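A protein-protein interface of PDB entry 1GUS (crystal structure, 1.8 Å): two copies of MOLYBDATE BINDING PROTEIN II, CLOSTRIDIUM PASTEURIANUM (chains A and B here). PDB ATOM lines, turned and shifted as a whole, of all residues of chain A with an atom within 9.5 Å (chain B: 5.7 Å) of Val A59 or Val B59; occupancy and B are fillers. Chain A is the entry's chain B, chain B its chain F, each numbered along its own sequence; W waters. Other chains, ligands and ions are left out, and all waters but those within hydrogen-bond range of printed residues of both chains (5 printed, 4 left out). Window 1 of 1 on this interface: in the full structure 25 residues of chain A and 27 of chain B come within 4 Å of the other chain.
Hydrophobic or aromatic side chains of chain B within 4 Å of the printed part of chain A: Leu B9, Ala B57, Val B58, Val B59, Val B64 and Met B65. Along chain B the printed residues that touch a printed residue of chain A span positions 6 to 65. Printed residues of chain A that touch a printed residue of chain B: Asn A7, Lys A34, Ile A35, Thr A36, Ser A37, Ile A38, Thr A56, Ala A57, Val A58, Val A59, Ser A61, Asp A63, Val A64, Met A65 and Leu A67. Among the printed residues, no Asp or Glu carboxylate lies within 4 Å of a Lys or Arg side-chain nitrogen of the other chain.
Water W4 lies within hydrogen-bond range of OD2 of Asp A63 (2.6 Å), O of Asp B63 (2.7 Å) and N of Lys A60 (2.9 Å). Water W1 lies within hydrogen-bond range of the backbone carbonyl oxygen of Lys A34, the backbone NH of Gln B8 and the backbone carbonyl oxygen of Arg B6.
The side-chain amide oxygen of Asn A7 is in hydrogen-bond range of the backbone NH of Thr B36. N of Thr A36 sits at hydrogen-bond distance from OD1 of Asn B7, at 2.6 Å. OG of Ser B61 lies within hydrogen-bond range of O of Thr A36 (3.3 Å). O of Val B64 is in hydrogen-bond range of OG of Ser A37, at 2.8 Å. The backbone NH (N) of Ile A38 is in hydrogen-bond range of the backbone carbonyl oxygen (O) of Ser B61 (3.0 Å). The backbone NH of Met B65 sits at hydrogen-bond distance from the backbone carbonyl oxygen of Val A58 (2.8 Å). OG of Ser A61 sits at hydrogen-bond distance from O of Thr B36, 3.4 Å away. N of Met A65 lies within hydrogen-bond range of O of Val B58 (3.0 Å).
Of the printed residues of chain B, Val A59 touches Val B59 (3.9 Å). Val B59 touches one residue of chain A. Val B58 touches four residues of chain A. Printed residues of chain A within 4 Å of Arg B6: Thr A36. Of the printed residues of chain B, Ser A37 touches Ser B61 and Val B64.
ND2 of Asn A7 sits at hydrogen-bond distance from O of Val A59 (2.9 Å). The backbone carbonyl oxygen of Leu A9 is in hydrogen-bond range of the backbone NH of Ala A57, at 2.8 Å. N of Leu A27 lies within hydrogen-bond range of O of Ile A35 (2.8 Å). The backbone NH (N) of Leu B9 is in hydrogen-bond range of the backbone carbonyl oxygen (O) of Ala B57 (2.8 Å).
Asn A7 touches Thr B36, and with the chains exchanged Thr A36 touches Asn B7. Thr A36 touches Ser B61, and with the chains exchanged Ser A61 touches Thr B36. Ala A57 touches Val B64, and with the chains exchanged Val A64 touches Ala B57. Ala A57 touches Met B65, and with the chains exchanged Met A65 touches Ala B57.
Among the printed residues, merely in contact across the chains: Lys A34 with Asn B7 (3.9 Å), Ile A35 with Asn B7 (3.0 Å), Ile A35 with Leu B9 (3.8 Å), Ile A35 with Val B64 (3.8 Å), Thr A36 with Arg B6 (3.99 Å), Thr A36 with Val B64 (3.5 Å), Ser A37 with Ser B61 (3.5 Å), Thr A56 with Met B65 (3.7 Å), Ala A57 with Val B64 (3.7 Å), Ala A57 with Met B65 (3.3 Å), Val A58 with Asp B63 (3.8 Å), Val A58 with Val B64 (3.7 Å), Val A59 with Val B59 (3.9 Å), Asp A63 with Val B58 (3.8 Å), Asp A63 with Asp B63 (3.4 Å), Val A64 with Thr B36 (3.6 Å), Val A64 with Ala B57 (3.8 Å), Val A64 with Val B58 (3.9 Å), Met A65 with Ala B57 (3.4 Å), Met A65 with Lys B60 (3.6 Å) and Leu A67 with Val B58 (3.9 Å).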
ATOM      1  N   ILE A   3      18.529 -10.602 -14.772  1.00  0.00           N
ATOM      2  CA  ILE A   3      17.923 -11.157 -15.972  1.00  0.00           C
ATOM      3  C   ILE A   3      17.719 -12.662 -15.803  1.00  0.00           C
ATOM      4  O   ILE A   3      18.458 -13.333 -15.070  1.00  0.00           O
ATOM      5  CB  ILE A   3      18.774 -10.776 -17.202  1.00  0.00           C
ATOM      6  CG1 ILE A   3      18.005 -11.028 -18.481  1.00  0.00           C
ATOM      7  CG2 ILE A   3      20.130 -11.488 -17.208  1.00  0.00           C
ATOM      8  CD1 ILE A   3      18.663 -10.327 -19.712  1.00  0.00           C
ATOM      9  N   SER A   4      16.723 -13.202 -16.493  1.00  0.00           N
ATOM     10  CA  SER A   4      16.402 -14.612 -16.368  1.00  0.00           C
ATOM     11  C   SER A   4      17.504 -15.539 -16.928  1.00  0.00           C
ATOM     12  O   SER A   4      17.572 -16.704 -16.583  1.00  0.00           O
ATOM     13  CB  SER A   4      15.036 -14.923 -17.050  1.00  0.00           C
ATOM     14  OG  SER A   4      15.090 -14.580 -18.416  1.00  0.00           O
ATOM     15  N   ALA A   5      18.361 -15.046 -17.813  1.00  0.00           N
ATOM     16  CA  ALA A   5      19.410 -15.897 -18.394  1.00  0.00           C
ATOM     17  C   ALA A   5      20.341 -16.327 -17.277  1.00  0.00           C
ATOM     18  O   ALA A   5      21.028 -15.506 -16.650  1.00  0.00           O
ATOM     19  CB  ALA A   5      20.162 -15.150 -19.504  1.00  0.00           C
ATOM     20  N   ARG A   6      20.330 -17.625 -16.985  1.00  0.00           N
ATOM     21  CA  ARG A   6      21.046 -18.131 -15.808  1.00  0.00           C
ATOM     22  C   ARG A   6      22.599 -18.205 -15.988  1.00  0.00           C
ATOM     23  O   ARG A   6      23.320 -18.422 -15.002  1.00  0.00           O
ATOM     24  CB  ARG A   6      20.505 -19.529 -15.437  1.00  0.00           C
ATOM     25  CG  ARG A   6      19.009 -19.491 -15.105  1.00  0.00           C
ATOM     26  CD  ARG A   6      18.516 -20.751 -14.393  1.00  0.00           C
ATOM     27  NE  ARG A   6      19.026 -20.855 -13.032  1.00  0.00           N
ATOM     28  CZ  ARG A   6      18.753 -19.997 -12.048  1.00  0.00           C
ATOM     29  NH1 ARG A   6      17.969 -18.948 -12.277  1.00  0.00           N
ATOM     30  NH2 ARG A   6      19.242 -20.214 -10.830  1.00  0.00           N
ATOM     31  N   ASN A   7      23.095 -18.167 -17.216  1.00  0.00           N
ATOM     32  CA  ASN A   7      24.513 -18.345 -17.418  1.00  0.00           C
ATOM     33  C   ASN A   7      25.151 -16.964 -17.527  1.00  0.00           C
ATOM     34  O   ASN A   7      24.753 -16.223 -18.414  1.00  0.00           O
ATOM     35  CB  ASN A   7      24.666 -19.110 -18.714  1.00  0.00           C
ATOM     36  CG  ASN A   7      24.007 -20.473 -18.628  1.00  0.00           C
ATOM     37  OD1 ASN A   7      24.452 -21.305 -17.863  1.00  0.00           O
ATOM     38  ND2 ASN A   7      22.935 -20.691 -19.382  1.00  0.00           N
ATOM     39  N   GLN A   8      26.055 -16.631 -16.604  1.00  0.00           N
ATOM     40  CA  GLN A   8      26.754 -15.328 -16.586  1.00  0.00           C
ATOM     41  C   GLN A   8      28.218 -15.599 -16.310  1.00  0.00           C
ATOM     42  O   GLN A   8      28.573 -15.886 -15.185  1.00  0.00           O
ATOM     43  CB  GLN A   8      26.167 -14.433 -15.475  1.00  0.00           C
ATOM     44  CG  GLN A   8      24.669 -14.084 -15.917  1.00  0.00           C
ATOM     45  CD  GLN A   8      23.880 -13.122 -15.045  1.00  0.00           C
ATOM     46  OE1 GLN A   8      24.438 -12.239 -14.380  1.00  0.00           O
ATOM     47  NE2 GLN A   8      22.561 -13.268 -15.075  1.00  0.00           N
ATOM     48  N   LEU A   9      29.043 -15.510 -17.344  1.00  0.00           N
ATOM     49  CA  LEU A   9      30.449 -15.941 -17.307  1.00  0.00           C
ATOM     50  C   LEU A   9      31.291 -14.700 -17.471  1.00  0.00           C
ATOM     51  O   LEU A   9      31.367 -14.121 -18.546  1.00  0.00           O
ATOM     52  CB  LEU A   9      30.702 -16.860 -18.493  1.00  0.00           C
ATOM     53  CG  LEU A   9      29.786 -18.102 -18.500  1.00  0.00           C
ATOM     54  CD1 LEU A   9      30.213 -18.983 -19.660  1.00  0.00           C
ATOM     55  CD2 LEU A   9      29.954 -18.873 -17.184  1.00  0.00           C
ATOM     56  N   LEU A  27      36.120 -13.862 -25.535  1.00  0.00           N
ATOM     57  CA  LEU A  27      36.370 -13.574 -24.121  1.00  0.00           C
ATOM     58  C   LEU A  27      37.083 -14.761 -23.531  1.00  0.00           C
ATOM     59  O   LEU A  27      36.702 -15.903 -23.758  1.00  0.00           O
ATOM     60  CB  LEU A  27      35.075 -13.408 -23.355  1.00  0.00           C
ATOM     61  CG  LEU A  27      34.048 -12.395 -23.816  1.00  0.00           C
ATOM     62  CD1 LEU A  27      32.844 -12.551 -22.849  1.00  0.00           C
ATOM     63  CD2 LEU A  27      34.636 -11.083 -23.528  1.00  0.00           C
ATOM     64  N   ILE A  29      37.581 -16.780 -20.231  1.00  0.00           N
ATOM     65  CA  ILE A  29      36.922 -16.866 -18.940  1.00  0.00           C
ATOM     66  C   ILE A  29      37.778 -17.701 -17.972  1.00  0.00           C
ATOM     67  O   ILE A  29      38.844 -18.176 -18.363  1.00  0.00           O
ATOM     68  CB  ILE A  29      35.513 -17.461 -19.057  1.00  0.00           C
ATOM     69  CG1 ILE A  29      35.537 -18.881 -19.600  1.00  0.00           C
ATOM     70  CG2 ILE A  29      34.623 -16.552 -19.925  1.00  0.00           C
ATOM     71  CD1 ILE A  29      34.156 -19.469 -19.626  1.00  0.00           C
ATOM     72  N   LYS A  34      37.495 -20.213 -23.566  1.00  0.00           N
ATOM     73  CA  LYS A  34      37.181 -19.019 -24.365  1.00  0.00           C
ATOM     74  C   LYS A  34      35.729 -19.116 -24.813  1.00  0.00           C
ATOM     75  O   LYS A  34      35.255 -20.216 -25.149  1.00  0.00           O
ATOM     76  CB  LYS A  34      38.083 -18.866 -25.602  1.00  0.00           C
ATOM     77  CG  LYS A  34      39.443 -18.165 -25.410  1.00  0.00           C
ATOM     78  CD  LYS A  34      40.356 -18.427 -26.608  1.00  0.00           C
ATOM     79  CE  LYS A  34      41.829 -17.995 -26.364  1.00  0.00           C
ATOM     80  NZ  LYS A  34      42.455 -17.270 -27.550  1.00  0.00           N
ATOM     81  N   ILE A  35      35.053 -17.977 -24.803  1.00  0.00           N
ATOM     82  CA  ILE A  35      33.657 -17.846 -25.212  1.00  0.00           C
ATOM     83  C   ILE A  35      33.688 -16.921 -26.407  1.00  0.00           C
ATOM     84  O   ILE A  35      34.417 -15.931 -26.410  1.00  0.00           O
ATOM     85  CB  ILE A  35      32.848 -17.147 -24.116  1.00  0.00           C
ATOM     86  CG1 ILE A  35      32.793 -17.991 -22.855  1.00  0.00           C
ATOM     87  CG2 ILE A  35      31.374 -16.839 -24.570  1.00  0.00           C
ATOM     88  CD1 ILE A  35      32.182 -19.348 -23.117  1.00  0.00           C
ATOM     89  N   THR A  36      32.958 -17.277 -27.453  1.00  0.00           N
ATOM     90  CA  THR A  36      32.890 -16.441 -28.646  1.00  0.00           C
ATOM     91  C   THR A  36      31.471 -15.982 -28.804  1.00  0.00           C
ATOM     92  O   THR A  36      30.560 -16.787 -28.712  1.00  0.00           O
ATOM     93  CB  THR A  36      33.249 -17.292 -29.851  1.00  0.00           C
ATOM     94  OG1 THR A  36      34.579 -17.758 -29.688  1.00  0.00           O
ATOM     95  CG2 THR A  36      33.303 -16.464 -31.170  1.00  0.00           C
ATOM     96  N   SER A  37      31.306 -14.682 -29.015  1.00  0.00           N
ATOM     97  CA  SER A  37      30.028 -14.031 -29.131  1.00  0.00           C
ATOM     98  C   SER A  37      29.945 -13.291 -30.478  1.00  0.00           C
ATOM     99  O   SER A  37      30.910 -12.660 -30.919  1.00  0.00           O
ATOM    100  CB  SER A  37      29.896 -13.019 -27.962  1.00  0.00           C
ATOM    101  OG  SER A  37      28.781 -12.143 -28.128  1.00  0.00           O
ATOM    102  N   ILE A  38      28.816 -13.396 -31.171  1.00  0.00           N
ATOM    103  CA  ILE A  38      28.587 -12.544 -32.345  1.00  0.00           C
ATOM    104  C   ILE A  38      27.376 -11.682 -31.998  1.00  0.00           C
ATOM    105  O   ILE A  38      26.263 -12.214 -31.762  1.00  0.00           O
ATOM    106  CB  ILE A  38      28.324 -13.382 -33.590  1.00  0.00           C
ATOM    107  CG1 ILE A  38      29.664 -14.014 -33.999  1.00  0.00           C
ATOM    108  CG2 ILE A  38      27.788 -12.513 -34.754  1.00  0.00           C
ATOM    109  CD1 ILE A  38      29.505 -15.127 -35.047  1.00  0.00           C
ATOM    110  N   THR A  56      30.920  -9.561 -19.287  1.00  0.00           N
ATOM    111  CA  THR A  56      30.340 -10.835 -18.854  1.00  0.00           C
ATOM    112  C   THR A  56      29.545 -11.438 -20.019  1.00  0.00           C
ATOM    113  O   THR A  56      28.777 -10.718 -20.663  1.00  0.00           O
ATOM    114  CB  THR A  56      29.394 -10.533 -17.720  1.00  0.00           C
ATOM    115  OG1 THR A  56      30.172 -10.076 -16.586  1.00  0.00           O
ATOM    116  CG2 THR A  56      28.725 -11.809 -17.225  1.00  0.00           C
ATOM    117  N   ALA A  57      29.692 -12.728 -20.294  1.00  0.00           N
ATOM    118  CA  ALA A  57      28.914 -13.379 -21.346  1.00  0.00           C
ATOM    119  C   ALA A  57      27.659 -13.959 -20.718  1.00  0.00           C
ATOM    120  O   ALA A  57      27.696 -14.524 -19.639  1.00  0.00           O
ATOM    121  CB  ALA A  57      29.769 -14.535 -21.949  1.00  0.00           C
ATOM    122  N   VAL A  58      26.540 -13.807 -21.406  1.00  0.00           N
ATOM    123  CA  VAL A  58      25.270 -14.247 -20.831  1.00  0.00           C
ATOM    124  C   VAL A  58      24.601 -15.111 -21.897  1.00  0.00           C
ATOM    125  O   VAL A  58      24.571 -14.751 -23.075  1.00  0.00           O
ATOM    126  CB  VAL A  58      24.376 -13.018 -20.603  1.00  0.00           C
ATOM    127  CG1 VAL A  58      22.989 -13.451 -20.098  1.00  0.00           C
ATOM    128  CG2 VAL A  58      25.083 -12.033 -19.614  1.00  0.00           C
ATOM    129  N   VAL A  59      24.085 -16.255 -21.459  1.00  0.00           N
ATOM    130  CA  VAL A  59      23.445 -17.149 -22.431  1.00  0.00           C
ATOM    131  C   VAL A  59      22.167 -17.705 -21.763  1.00  0.00           C
ATOM    132  O   VAL A  59      22.170 -18.170 -20.609  1.00  0.00           O
ATOM    133  CB  VAL A  59      24.331 -18.368 -22.696  1.00  0.00           C
ATOM    134  CG1 VAL A  59      23.633 -19.301 -23.710  1.00  0.00           C
ATOM    135  CG2 VAL A  59      25.736 -17.917 -23.258  1.00  0.00           C
ATOM    136  N   LYS A  60      21.074 -17.727 -22.531  1.00  0.00           N
ATOM    137  CA  LYS A  60      19.843 -18.260 -22.023  1.00  0.00           C
ATOM    138  C   LYS A  60      19.967 -19.755 -21.919  1.00  0.00           C
ATOM    139  O   LYS A  60      20.528 -20.384 -22.814  1.00  0.00           O
ATOM    140  CB  LYS A  60      18.701 -17.885 -23.024  1.00  0.00           C
ATOM    141  CG  LYS A  60      17.273 -18.154 -22.446  1.00  0.00           C
ATOM    142  CD  LYS A  60      16.156 -17.569 -23.368  1.00  0.00           C
ATOM    143  CE  LYS A  60      14.773 -17.586 -22.642  1.00  0.00           C
ATOM    144  NZ  LYS A  60      14.330 -19.071 -22.426  1.00  0.00           N
ATOM    145  N   SER A  61      19.407 -20.387 -20.873  1.00  0.00           N
ATOM    146  CA  SER A  61      19.576 -21.841 -20.757  1.00  0.00           C
ATOM    147  C   SER A  61      19.073 -22.704 -21.902  1.00  0.00           C
ATOM    148  O   SER A  61      19.671 -23.742 -22.200  1.00  0.00           O
ATOM    149  CB  SER A  61      18.833 -22.313 -19.483  1.00  0.00           C
ATOM    150  OG  SER A  61      19.327 -21.691 -18.283  1.00  0.00           O
ATOM    151  N   THR A  62      17.962 -22.312 -22.516  1.00  0.00           N
ATOM    152  CA  THR A  62      17.442 -23.009 -23.678  1.00  0.00           C
ATOM    153  C   THR A  62      18.368 -22.968 -24.904  1.00  0.00           C
ATOM    154  O   THR A  62      18.146 -23.684 -25.874  1.00  0.00           O
ATOM    155  CB  THR A  62      16.010 -22.454 -24.080  1.00  0.00           C
ATOM    156  OG1 THR A  62      16.032 -21.035 -24.113  1.00  0.00           O
ATOM    157  CG2 THR A  62      14.967 -22.721 -22.987  1.00  0.00           C
ATOM    158  N   ASP A  63      19.437 -22.157 -24.872  1.00  0.00           N
ATOM    159  CA  ASP A  63      20.387 -22.128 -25.982  1.00  0.00           C
ATOM    160  C   ASP A  63      21.617 -23.004 -25.716  1.00  0.00           C
ATOM    161  O   ASP A  63      22.548 -23.073 -26.511  1.00  0.00           O
ATOM    162  CB  ASP A  63      20.878 -20.696 -26.237  1.00  0.00           C
ATOM    163  CG  ASP A  63      19.777 -19.797 -26.921  1.00  0.00           C
ATOM    164  OD1 ASP A  63      18.846 -20.317 -27.584  1.00  0.00           O
ATOM    165  OD2 ASP A  63      19.814 -18.577 -26.732  1.00  0.00           O
ATOM    166  N   VAL A  64      21.664 -23.671 -24.573  1.00  0.00           N
ATOM    167  CA  VAL A  64      22.845 -24.477 -24.299  1.00  0.00           C
ATOM    168  C   VAL A  64      22.576 -25.916 -24.627  1.00  0.00           C
ATOM    169  O   VAL A  64      21.678 -26.512 -24.036  1.00  0.00           O
ATOM    170  CB  VAL A  64      23.174 -24.417 -22.781  1.00  0.00           C
ATOM    171  CG1 VAL A  64      24.400 -25.282 -22.502  1.00  0.00           C
ATOM    172  CG2 VAL A  64      23.365 -22.942 -22.342  1.00  0.00           C
ATOM    173  N   MET A  65      23.312 -26.467 -25.573  1.00  0.00           N
ATOM    174  CA  MET A  65      23.148 -27.870 -25.929  1.00  0.00           C
ATOM    175  C   MET A  65      24.116 -28.684 -25.106  1.00  0.00           C
ATOM    176  O   MET A  65      25.064 -28.148 -24.572  1.00  0.00           O
ATOM    177  CB  MET A  65      23.415 -28.088 -27.401  1.00  0.00           C
ATOM    178  CG  MET A  65      22.320 -27.462 -28.218  1.00  0.00           C
ATOM    179  SD  MET A  65      23.095 -27.087 -29.775  1.00  0.00           S
ATOM    180  CE  MET A  65      23.939 -25.379 -29.456  1.00  0.00           C
ATOM    181  N   ILE A  66      23.878 -29.993 -25.009  1.00  0.00           N
ATOM    182  CA  ILE A  66      24.773 -30.828 -24.239  1.00  0.00           C
ATOM    183  C   ILE A  66      25.390 -31.852 -25.202  1.00  0.00           C
ATOM    184  O   ILE A  66      24.674 -32.502 -25.950  1.00  0.00           O
ATOM    185  CB  ILE A  66      23.984 -31.524 -23.056  1.00  0.00           C
ATOM    186  CG1 ILE A  66      23.566 -30.526 -21.953  1.00  0.00           C
ATOM    187  CG2 ILE A  66      24.872 -32.616 -22.420  1.00  0.00           C
ATOM    188  CD1 ILE A  66      24.665 -29.681 -21.354  1.00  0.00           C
ATOM    189  N   LEU A  67      26.704 -32.016 -25.156  1.00  0.00           N
ATOM    190  CA  LEU A  67      27.421 -32.982 -25.999  1.00  0.00           C
ATOM    191  C   LEU A  67      28.024 -34.056 -25.104  1.00  0.00           C
ATOM    192  O   LEU A  67      28.613 -33.724 -24.080  1.00  0.00           O
ATOM    193  CB  LEU A  67      28.598 -32.280 -26.701  1.00  0.00           C
ATOM    194  CG  LEU A  67      29.693 -33.029 -27.479  1.00  0.00           C
ATOM    195  CD1 LEU A  67      29.155 -33.705 -28.722  1.00  0.00           C
ATOM    196  CD2 LEU A  67      30.895 -32.131 -27.899  1.00  0.00           C
ATOM    197  N   ALA B   5      29.651 -24.650 -33.733  1.00  0.00           N
ATOM    198  CA  ALA B   5      29.408 -23.865 -32.521  1.00  0.00           C
ATOM    199  C   ALA B   5      30.761 -23.661 -31.829  1.00  0.00           C
ATOM    200  O   ALA B   5      31.427 -24.604 -31.422  1.00  0.00           O
ATOM    201  CB  ALA B   5      28.381 -24.580 -31.611  1.00  0.00           C
ATOM    202  N   ARG B   6      31.187 -22.417 -31.714  1.00  0.00           N
ATOM    203  CA  ARG B   6      32.534 -22.177 -31.195  1.00  0.00           C
ATOM    204  C   ARG B   6      32.679 -22.234 -29.675  1.00  0.00           C
ATOM    205  O   ARG B   6      33.787 -22.118 -29.170  1.00  0.00           O
ATOM    206  CB  ARG B   6      33.059 -20.838 -31.712  1.00  0.00           C
ATOM    207  CG  ARG B   6      33.078 -20.799 -33.255  1.00  0.00           C
ATOM    208  CD  ARG B   6      33.937 -19.680 -33.813  1.00  0.00           C
ATOM    209  NE  ARG B   6      35.352 -19.785 -33.440  1.00  0.00           N
ATOM    210  CZ  ARG B   6      36.212 -20.606 -34.049  1.00  0.00           C
ATOM    211  NH1 ARG B   6      35.798 -21.393 -35.053  1.00  0.00           N
ATOM    212  NH2 ARG B   6      37.494 -20.647 -33.666  1.00  0.00           N
ATOM    213  N   ASN B   7      31.576 -22.388 -28.942  1.00  0.00           N
ATOM    214  CA  ASN B   7      31.709 -22.479 -27.497  1.00  0.00           C
ATOM    215  C   ASN B   7      31.522 -23.937 -27.101  1.00  0.00           C
ATOM    216  O   ASN B   7      30.431 -24.487 -27.327  1.00  0.00           O
ATOM    217  CB  ASN B   7      30.647 -21.611 -26.866  1.00  0.00           C
ATOM    218  CG  ASN B   7      30.841 -20.157 -27.253  1.00  0.00           C
ATOM    219  OD1 ASN B   7      31.817 -19.544 -26.818  1.00  0.00           O
ATOM    220  ND2 ASN B   7      29.980 -19.621 -28.120  1.00  0.00           N
ATOM    221  N   GLN B   8      32.569 -24.558 -26.563  1.00  0.00           N
ATOM    222  CA  GLN B   8      32.437 -25.984 -26.253  1.00  0.00           C
ATOM    223  C   GLN B   8      33.118 -26.091 -24.908  1.00  0.00           C
ATOM    224  O   GLN B   8      34.343 -26.108 -24.817  1.00  0.00           O
ATOM    225  CB  GLN B   8      33.112 -26.854 -27.363  1.00  0.00           C
ATOM    226  CG  GLN B   8      32.373 -26.737 -28.701  1.00  0.00           C
ATOM    227  CD  GLN B   8      32.998 -27.589 -29.807  1.00  0.00           C
ATOM    228  OE1 GLN B   8      33.663 -28.580 -29.517  1.00  0.00           O
ATOM    229  NE2 GLN B   8      32.825 -27.177 -31.071  1.00  0.00           N
ATOM    230  N   LEU B   9      32.337 -26.156 -23.842  1.00  0.00           N
ATOM    231  CA  LEU B   9      32.906 -26.061 -22.503  1.00  0.00           C
ATOM    232  C   LEU B   9      32.706 -27.396 -21.788  1.00  0.00           C
ATOM    233  O   LEU B   9      31.584 -27.840 -21.582  1.00  0.00           O
ATOM    234  CB  LEU B   9      32.163 -24.971 -21.744  1.00  0.00           C
ATOM    235  CG  LEU B   9      31.989 -23.677 -22.558  1.00  0.00           C
ATOM    236  CD1 LEU B   9      30.822 -22.853 -21.981  1.00  0.00           C
ATOM    237  CD2 LEU B   9      33.276 -22.945 -22.375  1.00  0.00           C
ATOM    238  N   THR B  36      23.868 -23.675 -17.048  1.00  0.00           N
ATOM    239  CA  THR B  36      22.583 -24.358 -16.950  1.00  0.00           C
ATOM    240  C   THR B  36      21.974 -24.486 -18.311  1.00  0.00           C
ATOM    241  O   THR B  36      22.028 -23.555 -19.093  1.00  0.00           O
ATOM    242  CB  THR B  36      21.646 -23.487 -16.081  1.00  0.00           C
ATOM    243  OG1 THR B  36      22.254 -23.460 -14.805  1.00  0.00           O
ATOM    244  CG2 THR B  36      20.329 -24.230 -15.825  1.00  0.00           C
ATOM    245  N   ALA B  57      29.154 -28.468 -22.802  1.00  0.00           N
ATOM    246  CA  ALA B  57      28.105 -27.502 -23.080  1.00  0.00           C
ATOM    247  C   ALA B  57      28.515 -26.789 -24.362  1.00  0.00           C
ATOM    248  O   ALA B  57      29.641 -26.356 -24.503  1.00  0.00           O
ATOM    249  CB  ALA B  57      27.990 -26.540 -21.957  1.00  0.00           C
ATOM    250  N   VAL B  58      27.579 -26.702 -25.286  1.00  0.00           N
ATOM    251  CA  VAL B  58      27.872 -26.165 -26.604  1.00  0.00           C
ATOM    252  C   VAL B  58      26.904 -25.038 -26.894  1.00  0.00           C
ATOM    253  O   VAL B  58      25.674 -25.232 -26.842  1.00  0.00           O
ATOM    254  CB  VAL B  58      27.725 -27.274 -27.699  1.00  0.00           C
ATOM    255  CG1 VAL B  58      27.976 -26.702 -29.081  1.00  0.00           C
ATOM    256  CG2 VAL B  58      28.705 -28.452 -27.461  1.00  0.00           C
ATOM    257  N   VAL B  59      27.452 -23.887 -27.287  1.00  0.00           N
ATOM    258  CA  VAL B  59      26.591 -22.767 -27.515  1.00  0.00           C
ATOM    259  C   VAL B  59      27.016 -22.097 -28.815  1.00  0.00           C
ATOM    260  O   VAL B  59      28.225 -21.908 -29.025  1.00  0.00           O
ATOM    261  CB  VAL B  59      26.732 -21.737 -26.396  1.00  0.00           C
ATOM    262  CG1 VAL B  59      25.811 -20.523 -26.663  1.00  0.00           C
ATOM    263  CG2 VAL B  59      26.333 -22.359 -24.991  1.00  0.00           C
ATOM    264  N   LYS B  60      26.037 -21.732 -29.638  1.00  0.00           N
ATOM    265  CA  LYS B  60      26.366 -21.032 -30.882  1.00  0.00           C
ATOM    266  C   LYS B  60      26.758 -19.593 -30.523  1.00  0.00           C
ATOM    267  O   LYS B  60      26.167 -18.973 -29.627  1.00  0.00           O
ATOM    268  CB  LYS B  60      25.154 -20.956 -31.836  1.00  0.00           C
ATOM    269  CG  LYS B  60      24.488 -22.270 -32.118  1.00  0.00           C
ATOM    270  CD  LYS B  60      23.144 -22.081 -32.964  1.00  0.00           C
ATOM    271  CE  LYS B  60      21.884 -21.931 -32.070  1.00  0.00           C
ATOM    272  NZ  LYS B  60      21.706 -23.152 -31.131  1.00  0.00           N
ATOM    273  N   SER B  61      27.735 -19.038 -31.254  1.00  0.00           N
ATOM    274  CA  SER B  61      28.180 -17.670 -30.974  1.00  0.00           C
ATOM    275  C   SER B  61      27.097 -16.610 -31.011  1.00  0.00           C
ATOM    276  O   SER B  61      27.113 -15.682 -30.208  1.00  0.00           O
ATOM    277  CB  SER B  61      29.299 -17.292 -31.994  1.00  0.00           C
ATOM    278  OG  SER B  61      30.421 -18.156 -31.751  1.00  0.00           O
ATOM    279  N   ASP B  63      24.200 -16.775 -29.977  1.00  0.00           N
ATOM    280  CA  ASP B  63      23.358 -16.780 -28.755  1.00  0.00           C
ATOM    281  C   ASP B  63      24.071 -16.232 -27.556  1.00  0.00           C
ATOM    282  O   ASP B  63      23.529 -16.184 -26.436  1.00  0.00           O
ATOM    283  CB  ASP B  63      23.000 -18.258 -28.427  1.00  0.00           C
ATOM    284  CG  ASP B  63      21.993 -18.802 -29.407  1.00  0.00           C
ATOM    285  OD1 ASP B  63      21.320 -17.933 -29.981  1.00  0.00           O
ATOM    286  OD2 ASP B  63      21.848 -19.999 -29.660  1.00  0.00           O
ATOM    287  N   VAL B  64      25.304 -15.807 -27.712  1.00  0.00           N
ATOM    288  CA  VAL B  64      25.973 -15.299 -26.492  1.00  0.00           C
ATOM    289  C   VAL B  64      25.831 -13.797 -26.448  1.00  0.00           C
ATOM    290  O   VAL B  64      26.256 -13.126 -27.399  1.00  0.00           O
ATOM    291  CB  VAL B  64      27.477 -15.608 -26.521  1.00  0.00           C
ATOM    292  CG1 VAL B  64      28.131 -15.041 -25.232  1.00  0.00           C
ATOM    293  CG2 VAL B  64      27.712 -17.171 -26.665  1.00  0.00           C
ATOM    294  N   MET B  65      25.266 -13.264 -25.377  1.00  0.00           N
ATOM    295  CA  MET B  65      25.157 -11.816 -25.221  1.00  0.00           C
ATOM    296  C   MET B  65      26.308 -11.307 -24.376  1.00  0.00           C
ATOM    297  O   MET B  65      26.960 -12.066 -23.649  1.00  0.00           O
ATOM    298  CB  MET B  65      23.816 -11.452 -24.551  1.00  0.00           C
ATOM    299  CG  MET B  65      22.663 -11.720 -25.448  1.00  0.00           C
ATOM    300  SD  MET B  65      21.139 -11.835 -24.501  1.00  0.00           S
ATOM    301  CE  MET B  65      21.342 -13.562 -23.752  1.00  0.00           C
HETATM  302  O   HOH W   1      34.775 -22.854 -25.932  1.00  0.00           O
HETATM  303  O   HOH W   2      24.311 -21.477 -14.665  1.00  0.00           O
HETATM  304  O   HOH W   3      20.479 -22.961 -12.302  1.00  0.00           O
HETATM  305  O   HOH W   4      21.150 -16.831 -25.260  1.00  0.00           O
HETATM  306  O   HOH W   5      23.285 -22.070 -28.908  1.00  0.00           O
